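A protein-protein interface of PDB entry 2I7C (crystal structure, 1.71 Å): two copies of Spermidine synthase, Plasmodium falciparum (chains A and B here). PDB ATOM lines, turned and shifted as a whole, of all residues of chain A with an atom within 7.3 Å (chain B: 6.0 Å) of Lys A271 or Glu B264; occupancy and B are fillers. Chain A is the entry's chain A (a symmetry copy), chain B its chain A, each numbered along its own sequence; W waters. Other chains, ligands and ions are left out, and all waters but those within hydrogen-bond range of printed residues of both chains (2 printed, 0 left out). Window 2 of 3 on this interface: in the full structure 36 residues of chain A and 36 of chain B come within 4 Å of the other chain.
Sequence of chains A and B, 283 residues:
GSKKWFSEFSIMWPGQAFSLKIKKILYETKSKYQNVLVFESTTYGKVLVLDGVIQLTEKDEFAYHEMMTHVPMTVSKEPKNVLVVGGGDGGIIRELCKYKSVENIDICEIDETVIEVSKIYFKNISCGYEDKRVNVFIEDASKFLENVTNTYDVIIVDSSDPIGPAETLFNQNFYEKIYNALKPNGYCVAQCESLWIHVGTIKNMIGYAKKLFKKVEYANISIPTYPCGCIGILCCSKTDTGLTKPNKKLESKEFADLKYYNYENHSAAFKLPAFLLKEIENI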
ATOM      1  N   LEU A 195      25.869   8.770   9.864  1.00  0.00           N
ATOM      2  CA  LEU A 195      26.264   9.120   8.497  1.00  0.00           C
ATOM      3  C   LEU A 195      27.694   8.652   8.147  1.00  0.00           C
ATOM      4  O   LEU A 195      28.046   8.542   6.977  1.00  0.00           O
ATOM      5  CB  LEU A 195      26.086  10.636   8.244  1.00  0.00           C
ATOM      6  CG  LEU A 195      26.769  11.701   9.118  1.00  0.00           C
ATOM      7  CD1 LEU A 195      28.242  11.895   8.732  1.00  0.00           C
ATOM      8  CD2 LEU A 195      26.013  13.036   8.999  1.00  0.00           C
ATOM      9  N   TYR A 218      16.859  14.713   6.649  1.00  0.00           N
ATOM     10  CA  TYR A 218      17.752  14.006   7.553  1.00  0.00           C
ATOM     11  C   TYR A 218      18.552  15.018   8.363  1.00  0.00           C
ATOM     12  O   TYR A 218      19.112  15.968   7.800  1.00  0.00           O
ATOM     13  CB  TYR A 218      18.674  13.096   6.743  1.00  0.00           C
ATOM     14  CG  TYR A 218      19.522  12.158   7.573  1.00  0.00           C
ATOM     15  CD1 TYR A 218      19.060  10.884   7.906  1.00  0.00           C
ATOM     16  CD2 TYR A 218      20.801  12.542   8.006  1.00  0.00           C
ATOM     17  CE1 TYR A 218      19.848  10.010   8.668  1.00  0.00           C
ATOM     18  CE2 TYR A 218      21.597  11.676   8.772  1.00  0.00           C
ATOM     19  CZ  TYR A 218      21.115  10.421   9.092  1.00  0.00           C
ATOM     20  OH  TYR A 218      21.899   9.586   9.839  1.00  0.00           O
ATOM     21  N   ALA A 219      18.584  14.824   9.683  1.00  0.00           N
ATOM     22  CA  ALA A 219      19.330  15.711  10.581  1.00  0.00           C
ATOM     23  C   ALA A 219      20.359  14.919  11.372  1.00  0.00           C
ATOM     24  O   ALA A 219      20.155  13.735  11.640  1.00  0.00           O
ATOM     25  CB  ALA A 219      18.380  16.444  11.532  1.00  0.00           C
ATOM     26  N   ASN A 220      21.444  15.579  11.765  1.00  0.00           N
ATOM     27  CA  ASN A 220      22.499  14.942  12.538  1.00  0.00           C
ATOM     28  C   ASN A 220      22.625  15.515  13.947  1.00  0.00           C
ATOM     29  O   ASN A 220      22.554  16.739  14.137  1.00  0.00           O
ATOM     30  CB  ASN A 220      23.848  15.085  11.811  1.00  0.00           C
ATOM     31  CG  ASN A 220      24.885  14.080  12.306  1.00  0.00           C
ATOM     32  OD1 ASN A 220      24.560  12.937  12.618  1.00  0.00           O
ATOM     33  ND2 ASN A 220      26.140  14.504  12.358  1.00  0.00           N
ATOM     34  N   THR A 244      12.586  21.421   8.985  1.00  0.00           N
ATOM     35  CA  THR A 244      13.854  22.140   9.210  1.00  0.00           C
ATOM     36  C   THR A 244      13.713  23.469   9.958  1.00  0.00           C
ATOM     37  O   THR A 244      14.699  23.993  10.495  1.00  0.00           O
ATOM     38  CB  THR A 244      14.655  22.385   7.899  1.00  0.00           C
ATOM     39  OG1 THR A 244      13.943  23.288   7.037  1.00  0.00           O
ATOM     40  CG2 THR A 244      14.935  21.067   7.177  1.00  0.00           C
ATOM     41  N   HIS A 266      18.347  23.787  15.705  1.00  0.00           N
ATOM     42  CA  HIS A 266      17.288  23.024  15.048  1.00  0.00           C
ATOM     43  C   HIS A 266      17.580  22.980  13.539  1.00  0.00           C
ATOM     44  O   HIS A 266      17.749  21.905  12.951  1.00  0.00           O
ATOM     45  CB  HIS A 266      15.928  23.684  15.356  1.00  0.00           C
ATOM     46  CG  HIS A 266      14.746  23.016  14.724  1.00  0.00           C
ATOM     47  ND1 HIS A 266      13.545  22.867  15.384  1.00  0.00           N
ATOM     48  CD2 HIS A 266      14.557  22.509  13.481  1.00  0.00           C
ATOM     49  CE1 HIS A 266      12.675  22.270  14.584  1.00  0.00           C
ATOM     50  NE2 HIS A 266      13.262  22.049  13.420  1.00  0.00           N
ATOM     51  N   SER A 267      17.678  24.156  12.920  1.00  0.00           N
ATOM     52  CA  SER A 267      17.889  24.248  11.480  1.00  0.00           C
ATOM     53  C   SER A 267      19.296  23.781  11.087  1.00  0.00           C
ATOM     54  O   SER A 267      19.482  23.160  10.038  1.00  0.00           O
ATOM     55  CB  SER A 267      17.606  25.671  10.996  1.00  0.00           C
ATOM     56  OG  SER A 267      16.274  26.053  11.315  1.00  0.00           O
ATOM     57  N   ALA A 268      20.284  24.064  11.942  1.00  0.00           N
ATOM     58  CA  ALA A 268      21.677  23.696  11.669  1.00  0.00           C
ATOM     59  C   ALA A 268      21.887  22.194  11.511  1.00  0.00           C
ATOM     60  O   ALA A 268      22.775  21.760  10.759  1.00  0.00           O
ATOM     61  CB  ALA A 268      22.600  24.247  12.757  1.00  0.00           C
ATOM     62  N   ALA A 269      21.070  21.400  12.222  1.00  0.00           N
ATOM     63  CA  ALA A 269      21.224  19.946  12.266  1.00  0.00           C
ATOM     64  C   ALA A 269      20.997  19.313  10.892  1.00  0.00           C
ATOM     65  O   ALA A 269      21.450  18.198  10.622  1.00  0.00           O
ATOM     66  CB  ALA A 269      20.248  19.345  13.302  1.00  0.00           C
ATOM     67  N   PHE A 270      20.290  20.048  10.031  1.00  0.00           N
ATOM     68  CA  PHE A 270      19.904  19.565   8.703  1.00  0.00           C
ATOM     69  C   PHE A 270      20.918  19.912   7.613  1.00  0.00           C
ATOM     70  O   PHE A 270      20.729  19.558   6.445  1.00  0.00           O
ATOM     71  CB  PHE A 270      18.519  20.094   8.323  1.00  0.00           C
ATOM     72  CG  PHE A 270      17.395  19.494   9.126  1.00  0.00           C
ATOM     73  CD1 PHE A 270      16.704  18.380   8.653  1.00  0.00           C
ATOM     74  CD2 PHE A 270      17.026  20.048  10.345  1.00  0.00           C
ATOM     75  CE1 PHE A 270      15.618  17.826   9.399  1.00  0.00           C
ATOM     76  CE2 PHE A 270      15.959  19.503  11.095  1.00  0.00           C
ATOM     77  CZ  PHE A 270      15.264  18.394  10.614  1.00  0.00           C
ATOM     78  N   LYS A 271      21.991  20.605   7.997  1.00  0.00           N
ATOM     79  CA  LYS A 271      23.025  21.010   7.050  1.00  0.00           C
ATOM     80  C   LYS A 271      24.094  19.913   7.065  1.00  0.00           C
ATOM     81  O   LYS A 271      24.897  19.815   7.986  1.00  0.00           O
ATOM     82  CB  LYS A 271      23.579  22.388   7.427  1.00  0.00           C
ATOM     83  CG  LYS A 271      22.521  23.492   7.476  1.00  0.00           C
ATOM     84  CD  LYS A 271      21.760  23.565   6.163  1.00  0.00           C
ATOM     85  CE  LYS A 271      20.725  24.686   6.138  1.00  0.00           C
ATOM     86  NZ  LYS A 271      20.006  24.704   4.812  1.00  0.00           N
ATOM     87  N   LEU A 272      24.034  19.044   6.066  1.00  0.00           N
ATOM     88  CA  LEU A 272      24.794  17.796   6.089  1.00  0.00           C
ATOM     89  C   LEU A 272      26.107  17.883   5.317  1.00  0.00           C
ATOM     90  O   LEU A 272      26.229  18.720   4.414  1.00  0.00           O
ATOM     91  CB  LEU A 272      23.951  16.668   5.511  1.00  0.00           C
ATOM     92  CG  LEU A 272      22.599  16.419   6.197  1.00  0.00           C
ATOM     93  CD1 LEU A 272      21.788  15.477   5.341  1.00  0.00           C
ATOM     94  CD2 LEU A 272      22.796  15.877   7.582  1.00  0.00           C
ATOM     95  N   PRO A 273      27.076  17.003   5.649  1.00  0.00           N
ATOM     96  CA  PRO A 273      28.364  16.974   4.923  1.00  0.00           C
ATOM     97  C   PRO A 273      28.163  16.668   3.439  1.00  0.00           C
ATOM     98  O   PRO A 273      27.215  15.953   3.070  1.00  0.00           O
ATOM     99  CB  PRO A 273      29.127  15.822   5.595  1.00  0.00           C
ATOM    100  CG  PRO A 273      28.468  15.644   6.926  1.00  0.00           C
ATOM    101  CD  PRO A 273      27.030  15.988   6.720  1.00  0.00           C
ATOM    102  N   ALA A 274      29.023  17.234   2.596  1.00  0.00           N
ATOM    103  CA  ALA A 274      28.891  17.112   1.143  1.00  0.00           C
ATOM    104  C   ALA A 274      28.725  15.669   0.648  1.00  0.00           C
ATOM    105  O   ALA A 274      27.873  15.409  -0.210  1.00  0.00           O
ATOM    106  CB  ALA A 274      30.056  17.814   0.419  1.00  0.00           C
ATOM    107  N   LEU A 277      25.061  14.340   1.093  1.00  0.00           N
ATOM    108  CA  LEU A 277      24.163  14.940   0.110  1.00  0.00           C
ATOM    109  C   LEU A 277      24.290  14.286  -1.266  1.00  0.00           C
ATOM    110  O   LEU A 277      23.288  14.024  -1.928  1.00  0.00           O
ATOM    111  CB  LEU A 277      24.378  16.449   0.037  1.00  0.00           C
ATOM    112  CG  LEU A 277      24.001  17.211   1.310  1.00  0.00           C
ATOM    113  CD1 LEU A 277      24.412  18.661   1.184  1.00  0.00           C
ATOM    114  CD2 LEU A 277      22.486  17.107   1.600  1.00  0.00           C
ATOM    115  N   ASN B 262      30.725  22.586   2.613  1.00  0.00           N
ATOM    116  CA  ASN B 262      30.000  23.372   1.616  1.00  0.00           C
ATOM    117  C   ASN B 262      29.551  24.710   2.199  1.00  0.00           C
ATOM    118  O   ASN B 262      29.748  24.982   3.383  1.00  0.00           O
ATOM    119  CB  ASN B 262      28.848  22.583   0.947  1.00  0.00           C
ATOM    120  CG  ASN B 262      27.810  22.072   1.937  1.00  0.00           C
ATOM    121  OD1 ASN B 262      27.405  22.771   2.869  1.00  0.00           O
ATOM    122  ND2 ASN B 262      27.366  20.837   1.722  1.00  0.00           N
ATOM    123  N   TYR B 263      28.964  25.543   1.351  1.00  0.00           N
ATOM    124  CA  TYR B 263      28.596  26.907   1.711  1.00  0.00           C
ATOM    125  C   TYR B 263      27.681  26.952   2.946  1.00  0.00           C
ATOM    126  O   TYR B 263      27.868  27.770   3.854  1.00  0.00           O
ATOM    127  CB  TYR B 263      27.920  27.554   0.498  1.00  0.00           C
ATOM    128  CG  TYR B 263      27.516  28.993   0.684  1.00  0.00           C
ATOM    129  CD1 TYR B 263      28.419  30.022   0.437  1.00  0.00           C
ATOM    130  CD2 TYR B 263      26.218  29.327   1.077  1.00  0.00           C
ATOM    131  CE1 TYR B 263      28.045  31.353   0.586  1.00  0.00           C
ATOM    132  CE2 TYR B 263      25.834  30.661   1.234  1.00  0.00           C
ATOM    133  CZ  TYR B 263      26.760  31.662   0.988  1.00  0.00           C
ATOM    134  OH  TYR B 263      26.409  32.990   1.129  1.00  0.00           O
ATOM    135  N   GLU B 264      26.705  26.049   2.970  1.00  0.00           N
ATOM    136  CA  GLU B 264      25.726  25.980   4.049  1.00  0.00           C
ATOM    137  C   GLU B 264      26.286  25.421   5.356  1.00  0.00           C
ATOM    138  O   GLU B 264      25.977  25.951   6.429  1.00  0.00           O
ATOM    139  CB  GLU B 264      24.498  25.197   3.591  1.00  0.00           C
ATOM    140  CG  GLU B 264      23.764  25.920   2.454  1.00  0.00           C
ATOM    141  CD  GLU B 264      22.275  25.780   2.542  1.00  0.00           C
ATOM    142  OE1 GLU B 264      21.791  24.643   2.755  1.00  0.00           O
ATOM    143  OE2 GLU B 264      21.585  26.813   2.393  1.00  0.00           O
ATOM    144  N   ASN B 265      27.103  24.366   5.280  1.00  0.00           N
ATOM    145  CA  ASN B 265      27.577  23.824   6.545  1.00  0.00           C
ATOM    146  C   ASN B 265      28.700  24.662   7.175  1.00  0.00           C
ATOM    147  O   ASN B 265      28.931  24.537   8.382  1.00  0.00           O
ATOM    148  CB  ASN B 265      27.780  22.290   6.557  1.00  0.00           C
ATOM    149  CG  ASN B 265      28.931  21.831   5.702  1.00  0.00           C
ATOM    150  OD1 ASN B 265      29.754  22.619   5.281  1.00  0.00           O
ATOM    151  ND2 ASN B 265      29.000  20.528   5.459  1.00  0.00           N
ATOM    152  N   HIS B 266      29.299  25.569   6.401  1.00  0.00           N
ATOM    153  CA  HIS B 266      30.222  26.564   6.943  1.00  0.00           C
ATOM    154  C   HIS B 266      29.535  27.282   8.116  1.00  0.00           C
ATOM    155  O   HIS B 266      30.015  27.249   9.256  1.00  0.00           O
ATOM    156  CB  HIS B 266      30.623  27.542   5.819  1.00  0.00           C
ATOM    157  CG  HIS B 266      31.555  28.636   6.239  1.00  0.00           C
ATOM    158  ND1 HIS B 266      32.589  29.069   5.437  1.00  0.00           N
ATOM    159  CD2 HIS B 266      31.580  29.423   7.342  1.00  0.00           C
ATOM    160  CE1 HIS B 266      33.230  30.057   6.043  1.00  0.00           C
ATOM    161  NE2 HIS B 266      32.632  30.297   7.197  1.00  0.00           N
ATOM    162  N   SER B 267      28.386  27.900   7.841  1.00  0.00           N
ATOM    163  CA  SER B 267      27.671  28.669   8.853  1.00  0.00           C
ATOM    164  C   SER B 267      27.070  27.759   9.931  1.00  0.00           C
ATOM    165  O   SER B 267      27.037  28.119  11.111  1.00  0.00           O
ATOM    166  CB  SER B 267      26.606  29.547   8.192  1.00  0.00           C
ATOM    167  OG  SER B 267      27.200  30.425   7.245  1.00  0.00           O
ATOM    168  N   ALA B 268      26.614  26.570   9.528  1.00  0.00           N
ATOM    169  CA  ALA B 268      25.992  25.620  10.458  1.00  0.00           C
ATOM    170  C   ALA B 268      26.920  25.178  11.583  1.00  0.00           C
ATOM    171  O   ALA B 268      26.459  24.884  12.698  1.00  0.00           O
ATOM    172  CB  ALA B 268      25.460  24.402   9.702  1.00  0.00           C
ATOM    173  N   ALA B 269      28.231  25.131  11.291  1.00  0.00           N
ATOM    174  CA  ALA B 269      29.230  24.617  12.228  1.00  0.00           C
ATOM    175  C   ALA B 269      29.321  25.481  13.486  1.00  0.00           C
ATOM    176  O   ALA B 269      29.785  25.030  14.536  1.00  0.00           O
ATOM    177  CB  ALA B 269      30.607  24.533  11.533  1.00  0.00           C
HETATM  178  O   HOH W   1      27.634  19.430   8.102  1.00  0.00           O
HETATM  179  O   HOH W   2      24.940  21.137   3.895  1.00  0.00           O
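Hydrophobic or aromatic side chains of chain A that line the printed part of chain B: Ala A268 and Leu A277.
Of the 8 printed residues of chain B, 4 touch a printed residue of chain A.
Hydrophobic or aromatic side chains of chain B within 4 Å of the printed part of chain A: Ala B268.
Among the printed residues, 7 pairs touch across the chains.
O of Ala B268 touches CB of Ala A268, at 3.9 Å.
Lys A271 touches Ala B268 (CB to CB, 3.6 Å).
Asn B262 touches Leu A272 (ND2 to O, 3.6 Å).
CA of Pro A273 touches ND2 of Asn B265 (3.7 Å).
Asn B262 touches Leu A277.
N of Asn B262 is in hydrogen-bond range of OD1 of Asn B265, 2.8 Å away.
N of Glu B264 sits close to OD1 of Asn B262 (3.4 Å).
Printed residues of chain B within 4 Å of Ala A268: Ala B268 (3.9 Å).
Ala A274 touches none of the printed residues of chain B.
Tyr B263 touches none of the printed residues of chain A.
Of the printed residues of chain A, Asn B265 touches Leu A272 (3.5 Å) and Pro A273 (3.7 Å).
The nearest printed residue of chain A that does not touch Asn B262 is Ala A274 (4.1 Å).
Ala A268 touches its own counterpart, Ala B268.
4 positions are printed for both chains.
Of the 7 pairs that touch across the chains among the printed residues, 1 has its exchanged pair printed and touching as well.
Water W1 lies within hydrogen-bond range of the backbone carbonyl oxygen of Lys A271 (2.8 Å) and the side-chain amide nitrogen of Asn B265 (3.2 Å).
Water W2 lies within hydrogen-bond range of O of Leu A272 (2.8 Å) and OD1 of Asn B262 (3.1 Å).
O of Leu A272 lies within hydrogen-bond range of ND2 of Asn B265, 3.5 Å away.
OE1 of Glu B264 is in salt-bridge range of NZ of Lys A271 (2.7 Å).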
